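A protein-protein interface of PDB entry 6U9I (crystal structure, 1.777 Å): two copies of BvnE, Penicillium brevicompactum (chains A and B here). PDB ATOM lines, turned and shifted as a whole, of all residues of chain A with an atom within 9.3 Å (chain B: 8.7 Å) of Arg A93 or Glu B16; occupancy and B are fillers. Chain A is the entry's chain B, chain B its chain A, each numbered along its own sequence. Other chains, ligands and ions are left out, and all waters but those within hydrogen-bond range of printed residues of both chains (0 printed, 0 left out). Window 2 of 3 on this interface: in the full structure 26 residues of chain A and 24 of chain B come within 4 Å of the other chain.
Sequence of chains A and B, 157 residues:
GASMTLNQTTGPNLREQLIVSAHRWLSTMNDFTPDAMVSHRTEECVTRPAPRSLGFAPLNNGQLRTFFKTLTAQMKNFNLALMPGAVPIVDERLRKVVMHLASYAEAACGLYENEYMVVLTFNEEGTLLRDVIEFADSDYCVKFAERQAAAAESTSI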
ATOM      1  N   LEU A  14     -18.807  15.282   1.513  1.00  0.00           N
ATOM      2  CA  LEU A  14     -17.691  14.356   1.351  1.00  0.00           C
ATOM      3  C   LEU A  14     -17.998  13.272   0.321  1.00  0.00           C
ATOM      4  O   LEU A  14     -17.130  12.911  -0.479  1.00  0.00           O
ATOM      5  CB  LEU A  14     -17.329  13.736   2.697  1.00  0.00           C
ATOM      6  CG  LEU A  14     -16.002  12.975   2.728  1.00  0.00           C
ATOM      7  CD1 LEU A  14     -14.862  13.842   2.189  1.00  0.00           C
ATOM      8  CD2 LEU A  14     -15.687  12.470   4.129  1.00  0.00           C
ATOM      9  N   ARG A  15     -19.223  12.740   0.312  1.00  0.00           N
ATOM     10  CA  ARG A  15     -19.522  11.689  -0.655  1.00  0.00           C
ATOM     11  C   ARG A  15     -19.350  12.191  -2.081  1.00  0.00           C
ATOM     12  O   ARG A  15     -18.758  11.500  -2.920  1.00  0.00           O
ATOM     13  CB  ARG A  15     -20.936  11.137  -0.450  1.00  0.00           C
ATOM     14  CG  ARG A  15     -21.247  10.003  -1.423  1.00  0.00           C
ATOM     15  CD  ARG A  15     -22.681   9.493  -1.315  1.00  0.00           C
ATOM     16  NE  ARG A  15     -22.853   8.306  -2.148  1.00  0.00           N
ATOM     17  CZ  ARG A  15     -22.765   7.057  -1.690  1.00  0.00           C
ATOM     18  NH1 ARG A  15     -22.908   6.033  -2.521  1.00  0.00           N
ATOM     19  NH2 ARG A  15     -22.522   6.838  -0.407  1.00  0.00           N
ATOM     20  N   LEU A  18     -15.577  12.563  -2.974  1.00  0.00           N
ATOM     21  CA  LEU A  18     -14.938  11.277  -3.233  1.00  0.00           C
ATOM     22  C   LEU A  18     -15.320  10.741  -4.610  1.00  0.00           C
ATOM     23  O   LEU A  18     -14.473  10.212  -5.339  1.00  0.00           O
ATOM     24  CB  LEU A  18     -15.310  10.289  -2.125  1.00  0.00           C
ATOM     25  CG  LEU A  18     -14.690  10.621  -0.756  1.00  0.00           C
ATOM     26  CD1 LEU A  18     -15.322   9.811   0.378  1.00  0.00           C
ATOM     27  CD2 LEU A  18     -13.181  10.406  -0.780  1.00  0.00           C
ATOM     28  N   VAL A  90     -19.032   4.049  -1.942  1.00  0.00           N
ATOM     29  CA  VAL A  90     -18.317   5.103  -1.223  1.00  0.00           C
ATOM     30  C   VAL A  90     -18.405   4.846   0.273  1.00  0.00           C
ATOM     31  O   VAL A  90     -19.505   4.764   0.835  1.00  0.00           O
ATOM     32  CB  VAL A  90     -18.865   6.498  -1.561  1.00  0.00           C
ATOM     33  CG1 VAL A  90     -18.053   7.570  -0.823  1.00  0.00           C
ATOM     34  CG2 VAL A  90     -18.807   6.730  -3.050  1.00  0.00           C
ATOM     35  N   ASP A  91     -17.248   4.746   0.922  1.00  0.00           N
ATOM     36  CA  ASP A  91     -17.139   4.724   2.374  1.00  0.00           C
ATOM     37  C   ASP A  91     -16.574   6.083   2.780  1.00  0.00           C
ATOM     38  O   ASP A  91     -15.364   6.312   2.678  1.00  0.00           O
ATOM     39  CB  ASP A  91     -16.241   3.574   2.834  1.00  0.00           C
ATOM     40  CG  ASP A  91     -16.175   3.444   4.350  1.00  0.00           C
ATOM     41  OD1 ASP A  91     -16.404   4.450   5.056  1.00  0.00           O
ATOM     42  OD2 ASP A  91     -15.892   2.326   4.846  1.00  0.00           O
ATOM     43  N   GLU A  92     -17.456   6.982   3.233  1.00  0.00           N
ATOM     44  CA  GLU A  92     -17.029   8.332   3.597  1.00  0.00           C
ATOM     45  C   GLU A  92     -16.084   8.319   4.789  1.00  0.00           C
ATOM     46  O   GLU A  92     -15.144   9.120   4.854  1.00  0.00           O
ATOM     47  CB  GLU A  92     -18.241   9.210   3.917  1.00  0.00           C
ATOM     48  CG  GLU A  92     -18.944   9.777   2.716  1.00  0.00           C
ATOM     49  CD  GLU A  92     -20.120  10.659   3.116  1.00  0.00           C
ATOM     50  OE1 GLU A  92     -19.922  11.607   3.907  1.00  0.00           O
ATOM     51  OE2 GLU A  92     -21.247  10.387   2.665  1.00  0.00           O
ATOM     52  N   ARG A  93     -16.323   7.434   5.755  1.00  0.00           N
ATOM     53  CA  ARG A  93     -15.472   7.420   6.944  1.00  0.00           C
ATOM     54  C   ARG A  93     -14.035   7.061   6.595  1.00  0.00           C
ATOM     55  O   ARG A  93     -13.088   7.669   7.116  1.00  0.00           O
ATOM     56  CB  ARG A  93     -16.011   6.440   7.983  1.00  0.00           C
ATOM     57  CG  ARG A  93     -15.223   6.487   9.282  1.00  0.00           C
ATOM     58  CD  ARG A  93     -15.670   5.461  10.305  1.00  0.00           C
ATOM     59  NE  ARG A  93     -16.949   5.799  10.926  1.00  0.00           N
ATOM     60  CZ  ARG A  93     -17.391   5.256  12.057  1.00  0.00           C
ATOM     61  NH1 ARG A  93     -18.568   5.610  12.554  1.00  0.00           N
ATOM     62  NH2 ARG A  93     -16.650   4.361  12.701  1.00  0.00           N
ATOM     63  N   LEU A  94     -13.851   6.061   5.737  1.00  0.00           N
ATOM     64  CA  LEU A  94     -12.522   5.591   5.364  1.00  0.00           C
ATOM     65  C   LEU A  94     -11.978   6.303   4.131  1.00  0.00           C
ATOM     66  O   LEU A  94     -10.833   6.040   3.741  1.00  0.00           O
ATOM     67  CB  LEU A  94     -12.544   4.072   5.126  1.00  0.00           C
ATOM     68  CG  LEU A  94     -12.959   3.170   6.296  1.00  0.00           C
ATOM     69  CD1 LEU A  94     -12.805   1.673   5.941  1.00  0.00           C
ATOM     70  CD2 LEU A  94     -12.193   3.511   7.579  1.00  0.00           C
ATOM     71  N   ARG A  95     -12.771   7.193   3.517  1.00  0.00           N
ATOM     72  CA  ARG A  95     -12.399   7.891   2.286  1.00  0.00           C
ATOM     73  C   ARG A  95     -12.047   6.905   1.175  1.00  0.00           C
ATOM     74  O   ARG A  95     -11.059   7.076   0.458  1.00  0.00           O
ATOM     75  CB  ARG A  95     -11.239   8.868   2.523  1.00  0.00           C
ATOM     76  CG  ARG A  95     -11.654  10.239   3.053  1.00  0.00           C
ATOM     77  CD  ARG A  95     -12.087  10.176   4.497  1.00  0.00           C
ATOM     78  NE  ARG A  95     -12.241  11.509   5.088  1.00  0.00           N
ATOM     79  CZ  ARG A  95     -12.762  11.727   6.289  1.00  0.00           C
ATOM     80  NH1 ARG A  95     -12.850  12.963   6.764  1.00  0.00           N
ATOM     81  NH2 ARG A  95     -13.196  10.708   7.017  1.00  0.00           N
ATOM     82  N   LYS A  96     -12.861   5.862   1.021  1.00  0.00           N
ATOM     83  CA  LYS A  96     -12.586   4.822   0.045  1.00  0.00           C
ATOM     84  C   LYS A  96     -13.691   4.785  -1.008  1.00  0.00           C
ATOM     85  O   LYS A  96     -14.857   5.063  -0.714  1.00  0.00           O
ATOM     86  CB  LYS A  96     -12.446   3.469   0.732  1.00  0.00           C
ATOM     87  CG  LYS A  96     -11.145   3.339   1.525  1.00  0.00           C
ATOM     88  CD  LYS A  96     -11.078   1.987   2.200  1.00  0.00           C
ATOM     89  CE  LYS A  96      -9.919   1.912   3.183  1.00  0.00           C
ATOM     90  NZ  LYS A  96      -8.610   1.721   2.484  1.00  0.00           N
ATOM     91  N   VAL A  97     -13.311   4.468  -2.243  1.00  0.00           N
ATOM     92  CA  VAL A  97     -14.267   4.283  -3.337  1.00  0.00           C
ATOM     93  C   VAL A  97     -13.932   2.973  -4.035  1.00  0.00           C
ATOM     94  O   VAL A  97     -12.780   2.758  -4.425  1.00  0.00           O
ATOM     95  CB  VAL A  97     -14.227   5.450  -4.345  1.00  0.00           C
ATOM     96  CG1 VAL A  97     -15.244   5.213  -5.477  1.00  0.00           C
ATOM     97  CG2 VAL A  97     -14.504   6.768  -3.647  1.00  0.00           C
ATOM     98  N   THR A 121      -8.310   4.717  -2.127  1.00  0.00           N
ATOM     99  CA  THR A 121      -8.351   5.381  -0.831  1.00  0.00           C
ATOM    100  C   THR A 121      -7.789   6.786  -1.003  1.00  0.00           C
ATOM    101  O   THR A 121      -6.736   6.966  -1.628  1.00  0.00           O
ATOM    102  CB  THR A 121      -7.551   4.612   0.233  1.00  0.00           C
ATOM    103  OG1 THR A 121      -7.990   3.247   0.291  1.00  0.00           O
ATOM    104  CG2 THR A 121      -7.732   5.259   1.620  1.00  0.00           C
ATOM    105  N   PHE A 122      -8.493   7.777  -0.467  1.00  0.00           N
ATOM    106  CA  PHE A 122      -8.098   9.170  -0.610  1.00  0.00           C
ATOM    107  C   PHE A 122      -7.636   9.736   0.724  1.00  0.00           C
ATOM    108  O   PHE A 122      -7.837   9.143   1.788  1.00  0.00           O
ATOM    109  CB  PHE A 122      -9.255   9.992  -1.181  1.00  0.00           C
ATOM    110  CG  PHE A 122      -9.613   9.594  -2.578  1.00  0.00           C
ATOM    111  CD1 PHE A 122     -10.529   8.569  -2.817  1.00  0.00           C
ATOM    112  CD2 PHE A 122      -9.003  10.205  -3.654  1.00  0.00           C
ATOM    113  CE1 PHE A 122     -10.832   8.192  -4.109  1.00  0.00           C
ATOM    114  CE2 PHE A 122      -9.309   9.833  -4.943  1.00  0.00           C
ATOM    115  CZ  PHE A 122     -10.217   8.818  -5.173  1.00  0.00           C
ATOM    116  N   ASN A 123      -7.008  10.910   0.653  1.00  0.00           N
ATOM    117  CA  ASN A 123      -6.676  11.636   1.868  1.00  0.00           C
ATOM    118  C   ASN A 123      -7.965  12.076   2.562  1.00  0.00           C
ATOM    119  O   ASN A 123      -9.076  11.843   2.083  1.00  0.00           O
ATOM    120  CB  ASN A 123      -5.749  12.818   1.560  1.00  0.00           C
ATOM    121  CG  ASN A 123      -6.354  13.836   0.587  1.00  0.00           C
ATOM    122  OD1 ASN A 123      -7.473  13.679   0.098  1.00  0.00           O
ATOM    123  ND2 ASN A 123      -5.605  14.907   0.325  1.00  0.00           N
ATOM    124  N   GLU A 124      -7.823  12.722   3.717  1.00  0.00           N
ATOM    125  CA  GLU A 124      -9.008  12.990   4.525  1.00  0.00           C
ATOM    126  C   GLU A 124      -9.926  14.016   3.870  1.00  0.00           C
ATOM    127  O   GLU A 124     -11.147  13.970   4.072  1.00  0.00           O
ATOM    128  CB  GLU A 124      -8.584  13.412   5.937  1.00  0.00           C
ATOM    129  CG  GLU A 124      -8.390  12.182   6.812  1.00  0.00           C
ATOM    130  CD  GLU A 124      -7.514  12.415   8.017  1.00  0.00           C
ATOM    131  OE1 GLU A 124      -6.540  11.646   8.207  1.00  0.00           O
ATOM    132  OE2 GLU A 124      -7.812  13.350   8.785  1.00  0.00           O
ATOM    133  N   GLU A 125      -9.375  14.920   3.060  1.00  0.00           N
ATOM    134  CA  GLU A 125     -10.197  15.874   2.322  1.00  0.00           C
ATOM    135  C   GLU A 125     -10.902  15.236   1.131  1.00  0.00           C
ATOM    136  O   GLU A 125     -11.824  15.844   0.566  1.00  0.00           O
ATOM    137  CB  GLU A 125      -9.325  17.038   1.846  1.00  0.00           C
ATOM    138  CG  GLU A 125     -10.079  18.287   1.423  1.00  0.00           C
ATOM    139  CD  GLU A 125      -9.160  19.495   1.277  1.00  0.00           C
ATOM    140  OE1 GLU A 125      -9.214  20.174   0.225  1.00  0.00           O
ATOM    141  OE2 GLU A 125      -8.382  19.760   2.217  1.00  0.00           O
ATOM    142  N   ARG A 130      -4.291   8.193  -2.173  1.00  0.00           N
ATOM    143  CA  ARG A 130      -3.177   7.696  -1.378  1.00  0.00           C
ATOM    144  C   ARG A 130      -3.021   6.182  -1.388  1.00  0.00           C
ATOM    145  O   ARG A 130      -1.985   5.685  -0.923  1.00  0.00           O
ATOM    146  CB  ARG A 130      -3.284   8.190   0.075  1.00  0.00           C
ATOM    147  CG  ARG A 130      -4.387   7.578   0.908  1.00  0.00           C
ATOM    148  CD  ARG A 130      -4.343   8.155   2.327  1.00  0.00           C
ATOM    149  NE  ARG A 130      -5.252   7.483   3.255  1.00  0.00           N
ATOM    150  CZ  ARG A 130      -4.998   6.312   3.832  1.00  0.00           C
ATOM    151  NH1 ARG A 130      -3.862   5.678   3.564  1.00  0.00           N
ATOM    152  NH2 ARG A 130      -5.880   5.768   4.667  1.00  0.00           N
ATOM    153  N   ASN B  13     -26.823   4.267  13.724  1.00  0.00           N
ATOM    154  CA  ASN B  13     -25.693   3.346  13.671  1.00  0.00           C
ATOM    155  C   ASN B  13     -25.875   2.279  12.581  1.00  0.00           C
ATOM    156  O   ASN B  13     -25.744   1.076  12.835  1.00  0.00           O
ATOM    157  CB  ASN B  13     -25.471   2.680  15.039  1.00  0.00           C
ATOM    158  CG  ASN B  13     -25.210   3.689  16.161  1.00  0.00           C
ATOM    159  OD1 ASN B  13     -25.989   3.790  17.109  1.00  0.00           O
ATOM    160  ND2 ASN B  13     -24.106   4.429  16.060  1.00  0.00           N
ATOM    161  N   LEU B  14     -26.169   2.730  11.360  1.00  0.00           N
ATOM    162  CA  LEU B  14     -26.303   1.795  10.250  1.00  0.00           C
ATOM    163  C   LEU B  14     -24.959   1.204   9.833  1.00  0.00           C
ATOM    164  O   LEU B  14     -24.891   0.028   9.451  1.00  0.00           O
ATOM    165  CB  LEU B  14     -26.968   2.484   9.071  1.00  0.00           C
ATOM    166  CG  LEU B  14     -27.238   1.547   7.902  1.00  0.00           C
ATOM    167  CD1 LEU B  14     -28.358   0.580   8.238  1.00  0.00           C
ATOM    168  CD2 LEU B  14     -27.601   2.378   6.688  1.00  0.00           C
ATOM    169  N   ARG B  15     -23.884   1.992   9.894  1.00  0.00           N
ATOM    170  CA  ARG B  15     -22.564   1.454   9.577  1.00  0.00           C
ATOM    171  C   ARG B  15     -22.227   0.268  10.472  1.00  0.00           C
ATOM    172  O   ARG B  15     -21.755  -0.770   9.999  1.00  0.00           O
ATOM    173  CB  ARG B  15     -21.496   2.537   9.715  1.00  0.00           C
ATOM    174  CG  ARG B  15     -20.094   2.009   9.475  1.00  0.00           C
ATOM    175  CD  ARG B  15     -19.012   3.052   9.757  1.00  0.00           C
ATOM    176  NE  ARG B  15     -17.713   2.591   9.269  1.00  0.00           N
ATOM    177  CZ  ARG B  15     -17.292   2.775   8.024  1.00  0.00           C
ATOM    178  NH1 ARG B  15     -18.070   3.418   7.150  1.00  0.00           N
ATOM    179  NH2 ARG B  15     -16.104   2.310   7.648  1.00  0.00           N
ATOM    180  N   GLU B  16     -22.455   0.400  11.778  1.00  0.00           N
ATOM    181  CA  GLU B  16     -22.113  -0.704  12.666  1.00  0.00           C
ATOM    182  C   GLU B  16     -22.987  -1.921  12.389  1.00  0.00           C
ATOM    183  O   GLU B  16     -22.500  -3.056  12.415  1.00  0.00           O
ATOM    184  CB  GLU B  16     -22.212  -0.258  14.129  1.00  0.00           C
ATOM    185  CG  GLU B  16     -21.244   0.880  14.498  1.00  0.00           C
ATOM    186  CD  GLU B  16     -21.668   2.247  13.952  1.00  0.00           C
ATOM    187  OE1 GLU B  16     -22.794   2.362  13.421  1.00  0.00           O
ATOM    188  OE2 GLU B  16     -20.871   3.206  14.051  1.00  0.00           O
ATOM    189  N   GLN B  17     -24.271  -1.702  12.089  1.00  0.00           N
ATOM    190  CA  GLN B  17     -25.152  -2.811  11.733  1.00  0.00           C
ATOM    191  C   GLN B  17     -24.648  -3.547  10.494  1.00  0.00           C
ATOM    192  O   GLN B  17     -24.693  -4.781  10.440  1.00  0.00           O
ATOM    193  CB  GLN B  17     -26.570  -2.305  11.489  1.00  0.00           C
ATOM    194  CG  GLN B  17     -27.502  -3.362  10.885  1.00  0.00           C
ATOM    195  CD  GLN B  17     -27.843  -4.478  11.859  1.00  0.00           C
ATOM    196  OE1 GLN B  17     -28.835  -4.396  12.579  1.00  0.00           O
ATOM    197  NE2 GLN B  17     -27.026  -5.532  11.881  1.00  0.00           N
ATOM    198  N   LEU B  18     -24.185  -2.805   9.481  1.00  0.00           N
ATOM    199  CA  LEU B  18     -23.699  -3.457   8.265  1.00  0.00           C
ATOM    200  C   LEU B  18     -22.417  -4.236   8.540  1.00  0.00           C
ATOM    201  O   LEU B  18     -22.214  -5.329   7.994  1.00  0.00           O
ATOM    202  CB  LEU B  18     -23.495  -2.418   7.157  1.00  0.00           C
ATOM    203  CG  LEU B  18     -24.794  -1.807   6.597  1.00  0.00           C
ATOM    204  CD1 LEU B  18     -24.522  -0.505   5.845  1.00  0.00           C
ATOM    205  CD2 LEU B  18     -25.520  -2.811   5.676  1.00  0.00           C
ATOM    206  N   ILE B  19     -21.554  -3.707   9.412  1.00  0.00           N
ATOM    207  CA  ILE B  19     -20.340  -4.430   9.773  1.00  0.00           C
ATOM    208  C   ILE B  19     -20.681  -5.703  10.538  1.00  0.00           C
ATOM    209  O   ILE B  19     -20.102  -6.764  10.287  1.00  0.00           O
ATOM    210  CB  ILE B  19     -19.392  -3.508  10.567  1.00  0.00           C
ATOM    211  CG1 ILE B  19     -18.843  -2.424   9.637  1.00  0.00           C
ATOM    212  CG2 ILE B  19     -18.268  -4.323  11.233  1.00  0.00           C
ATOM    213  CD1 ILE B  19     -17.944  -1.395  10.304  1.00  0.00           C
ATOM    214  N   VAL B  20     -21.646  -5.628  11.466  1.00  0.00           N
ATOM    215  CA  VAL B  20     -22.093  -6.819  12.186  1.00  0.00           C
ATOM    216  C   VAL B  20     -22.648  -7.862  11.222  1.00  0.00           C
ATOM    217  O   VAL B  20     -22.342  -9.056  11.336  1.00  0.00           O
ATOM    218  CB  VAL B  20     -23.123  -6.435  13.266  1.00  0.00           C
ATOM    219  CG1 VAL B  20     -23.893  -7.656  13.730  1.00  0.00           C
ATOM    220  CG2 VAL B  20     -22.420  -5.749  14.439  1.00  0.00           C
ATOM    221  N   SER B  21     -23.464  -7.442  10.248  1.00  0.00           N
ATOM    222  CA  SER B  21     -23.992  -8.435   9.309  1.00  0.00           C
ATOM    223  C   SER B  21     -22.927  -8.974   8.365  1.00  0.00           C
ATOM    224  O   SER B  21     -23.012 -10.138   7.953  1.00  0.00           O
ATOM    225  CB  SER B  21     -25.174  -7.883   8.508  1.00  0.00           C
ATOM    226  OG  SER B  21     -26.141  -7.314   9.363  1.00  0.00           O
ATOM    227  N   ALA B  22     -21.933  -8.158   7.994  1.00  0.00           N
ATOM    228  CA  ALA B  22     -20.841  -8.687   7.181  1.00  0.00           C
ATOM    229  C   ALA B  22     -20.016  -9.697   7.969  1.00  0.00           C
ATOM    230  O   ALA B  22     -19.617 -10.742   7.438  1.00  0.00           O
ATOM    231  CB  ALA B  22     -19.949  -7.549   6.674  1.00  0.00           C
ATOM    232  N   HIS B  23     -19.745  -9.412   9.245  1.00  0.00           N
ATOM    233  CA  HIS B  23     -19.015 -10.394  10.036  1.00  0.00           C
ATOM    234  C   HIS B  23     -19.855 -11.631  10.298  1.00  0.00           C
ATOM    235  O   HIS B  23     -19.310 -12.739  10.380  1.00  0.00           O
ATOM    236  CB  HIS B  23     -18.530  -9.765  11.343  1.00  0.00           C
ATOM    237  CG  HIS B  23     -17.294  -8.933  11.173  1.00  0.00           C
ATOM    238  ND1 HIS B  23     -16.094  -9.467  10.751  1.00  0.00           N
ATOM    239  CD2 HIS B  23     -17.076  -7.608  11.344  1.00  0.00           C
ATOM    240  CE1 HIS B  23     -15.190  -8.504  10.675  1.00  0.00           C
ATOM    241  NE2 HIS B  23     -15.761  -7.367  11.028  1.00  0.00           N
ATOM    242  N   PRO B  88     -13.411  -4.222   6.535  1.00  0.00           N
ATOM    243  CA  PRO B  88     -14.604  -3.999   5.708  1.00  0.00           C
ATOM    244  C   PRO B  88     -14.749  -2.541   5.296  1.00  0.00           C
ATOM    245  O   PRO B  88     -14.530  -1.620   6.085  1.00  0.00           O
ATOM    246  CB  PRO B  88     -15.756  -4.443   6.618  1.00  0.00           C
ATOM    247  CG  PRO B  88     -15.127  -5.376   7.596  1.00  0.00           C
ATOM    248  CD  PRO B  88     -13.753  -4.812   7.842  1.00  0.00           C
ATOM    249  N   ILE B  89     -15.151  -2.341   4.047  1.00  0.00           N
ATOM    250  CA  ILE B  89     -15.397  -1.022   3.476  1.00  0.00           C
ATOM    251  C   ILE B  89     -16.903  -0.893   3.367  1.00  0.00           C
ATOM    252  O   ILE B  89     -17.540  -1.737   2.739  1.00  0.00           O
ATOM    253  CB  ILE B  89     -14.736  -0.882   2.098  1.00  0.00           C
ATOM    254  CG1 ILE B  89     -13.241  -1.180   2.202  1.00  0.00           C
ATOM    255  CG2 ILE B  89     -14.997   0.497   1.514  1.00  0.00           C
ATOM    256  CD1 ILE B  89     -12.580  -1.334   0.851  1.00  0.00           C
ATOM    257  N   VAL B  90     -17.483   0.141   3.979  1.00  0.00           N
ATOM    258  CA  VAL B  90     -18.933   0.202   4.177  1.00  0.00           C
ATOM    259  C   VAL B  90     -19.501   1.441   3.498  1.00  0.00           C
ATOM    260  O   VAL B  90     -19.109   2.569   3.831  1.00  0.00           O
ATOM    261  CB  VAL B  90     -19.304   0.203   5.667  1.00  0.00           C
ATOM    262  CG1 VAL B  90     -20.833   0.196   5.826  1.00  0.00           C
ATOM    263  CG2 VAL B  90     -18.694  -0.999   6.357  1.00  0.00           C
ATOM    264  N   ASP B  91     -20.466   1.237   2.581  1.00  0.00           N
ATOM    265  CA  ASP B  91     -21.256   2.324   1.997  1.00  0.00           C
ATOM    266  C   ASP B  91     -22.644   2.244   2.625  1.00  0.00           C
ATOM    267  O   ASP B  91     -23.482   1.452   2.185  1.00  0.00           O
ATOM    268  CB  ASP B  91     -21.317   2.213   0.474  1.00  0.00           C
ATOM    269  CG  ASP B  91     -22.015   3.419  -0.192  1.00  0.00           C
ATOM    270  OD1 ASP B  91     -22.771   4.136   0.489  1.00  0.00           O
ATOM    271  OD2 ASP B  91     -21.819   3.644  -1.410  1.00  0.00           O
ATOM    272  N   GLU B  92     -22.880   3.067   3.657  1.00  0.00           N
ATOM    273  CA  GLU B  92     -24.161   3.044   4.365  1.00  0.00           C
ATOM    274  C   GLU B  92     -25.323   3.354   3.434  1.00  0.00           C
ATOM    275  O   GLU B  92     -26.398   2.756   3.549  1.00  0.00           O
ATOM    276  CB  GLU B  92     -24.160   4.066   5.500  1.00  0.00           C
ATOM    277  CG  GLU B  92     -23.538   3.610   6.776  1.00  0.00           C
ATOM    278  CD  GLU B  92     -23.710   4.647   7.874  1.00  0.00           C
ATOM    279  OE1 GLU B  92     -22.697   5.249   8.290  1.00  0.00           O
ATOM    280  OE2 GLU B  92     -24.867   4.874   8.303  1.00  0.00           O
ATOM    281  N   VAL B  97     -21.149  -3.648   1.654  1.00  0.00           N
ATOM    282  CA  VAL B  97     -19.891  -3.879   2.371  1.00  0.00           C
ATOM    283  C   VAL B  97     -18.943  -4.611   1.433  1.00  0.00           C
ATOM    284  O   VAL B  97     -19.296  -5.667   0.897  1.00  0.00           O
ATOM    285  CB  VAL B  97     -20.090  -4.701   3.658  1.00  0.00           C
ATOM    286  CG1 VAL B  97     -18.724  -4.921   4.365  1.00  0.00           C
ATOM    287  CG2 VAL B  97     -21.073  -4.000   4.590  1.00  0.00           C
ATOM    288  N   GLU B 125     -32.786  -2.549   5.888  1.00  0.00           N
ATOM    289  CA  GLU B 125     -32.535  -2.595   7.319  1.00  0.00           C
ATOM    290  C   GLU B 125     -31.126  -3.062   7.648  1.00  0.00           C
ATOM    291  O   GLU B 125     -30.720  -2.990   8.816  1.00  0.00           O
ATOM    292  CB  GLU B 125     -33.548  -3.517   8.000  1.00  0.00           C
ATOM    293  CG  GLU B 125     -35.000  -3.258   7.588  1.00  0.00           C
ATOM    294  CD  GLU B 125     -35.482  -4.202   6.483  1.00  0.00           C
ATOM    295  OE1 GLU B 125     -35.179  -3.962   5.292  1.00  0.00           O
ATOM    296  OE2 GLU B 125     -36.175  -5.191   6.813  1.00  0.00           O
ATOM    297  N   GLY B 126     -30.383  -3.545   6.653  1.00  0.00           N
ATOM    298  CA  GLY B 126     -29.039  -4.044   6.882  1.00  0.00           C
ATOM    299  C   GLY B 126     -28.961  -5.369   7.602  1.00  0.00           C
ATOM    300  O   GLY B 126     -27.916  -5.686   8.172  1.00  0.00           O
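Among the printed residues, merely in contact across the chains: Val A90 with Val B90 (3.7 Å), Asp A91 with Ile B89 (3.6 Å), Arg A93 with Arg B15 (3.6 Å), Leu A94 with Arg B15 (3.5 Å), Leu A94 with Pro B88 (3.7 Å) and Lys A96 with Ile B89 (3.8 Å).
OE2 of Glu B16 is in salt-bridge range of NH1 of Arg A93, at 3.7 Å.
The guanidinium group of Arg B15 is in salt-bridge range of the side-chain carboxylate of Asp A91.
The side-chain carboxylate (OD2) of Asp B91 is in hydrogen-bond range of the backbone NH (N) of Val A90, at 2.9 Å.
OD2 of Asp B91 is in salt-bridge range of NH1 of Arg A15, at 2.9 Å.
The backbone NH (N) of Val B90 sits at hydrogen-bond distance from the side-chain carboxylate (OD2) of Asp A91 (2.8 Å).
Arg A93 touches two residues of chain B.
Printed residues of chain B within 4 Å of Lys A96: Ile B89 (3.8 Å).
No residue of chain A comes within 4 Å of Asn B13.
Glu B16 touches just one residue of chain A: Arg A93.
No residue of chain A comes within 4 Å of Ile B19.
Printed residues of chain A within 4 Å of Pro B88: Leu A94.
Of the printed residues of chain A, Val B90 touches Val A90 and Asp A91.
The nearest printed residue of chain B that does not touch Arg A93 is Val B90 (5.9 Å).
The nearest printed residue of chain A that does not touch Glu B16 is Asp A91 (9.7 Å).
The guanidinium group (NH2) of Arg A95 sits at hydrogen-bond distance from the backbone carbonyl oxygen (O) of Arg A93 (3.0 Å).
O of Lys A96 sits at hydrogen-bond distance from N of Asp A91 (2.9 Å).
The side-chain carboxylate (OD1) of Asp A91 lies within hydrogen-bond range of the backbone NH (N) of Leu A94, at 3.1 Å.
N of Arg B15 lies close to OE2 of Glu B92, at 3.4 Å.
The backbone NH (N) of Arg A93 lies within hydrogen-bond range of the side-chain carboxylate (OD1) of Asp A91, 3.1 Å away.
The side-chain amino group of Lys A96 is in hydrogen-bond range of the side-chain hydroxyl of Thr A121 (2.7 Å).
Of the 17 printed residues of chain A, 6 touch a printed residue of chain B.
Hydrophobic or aromatic side chains of chain B within 4 Å of the printed part of chain A: Ile B89.
Among the printed residues, 11 pairs touch across the chains.
Arg A15 touches Asp B91, and with the chains exchanged Asp A91 touches Arg B15.
Val B90 touches its own counterpart, Val A90.
Val A90 touches Asp B91, and with the chains exchanged Asp A91 touches Val B90.
Positions printed for both chains: 14, 15, 18, 90, 91, 92, 97 and 125.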
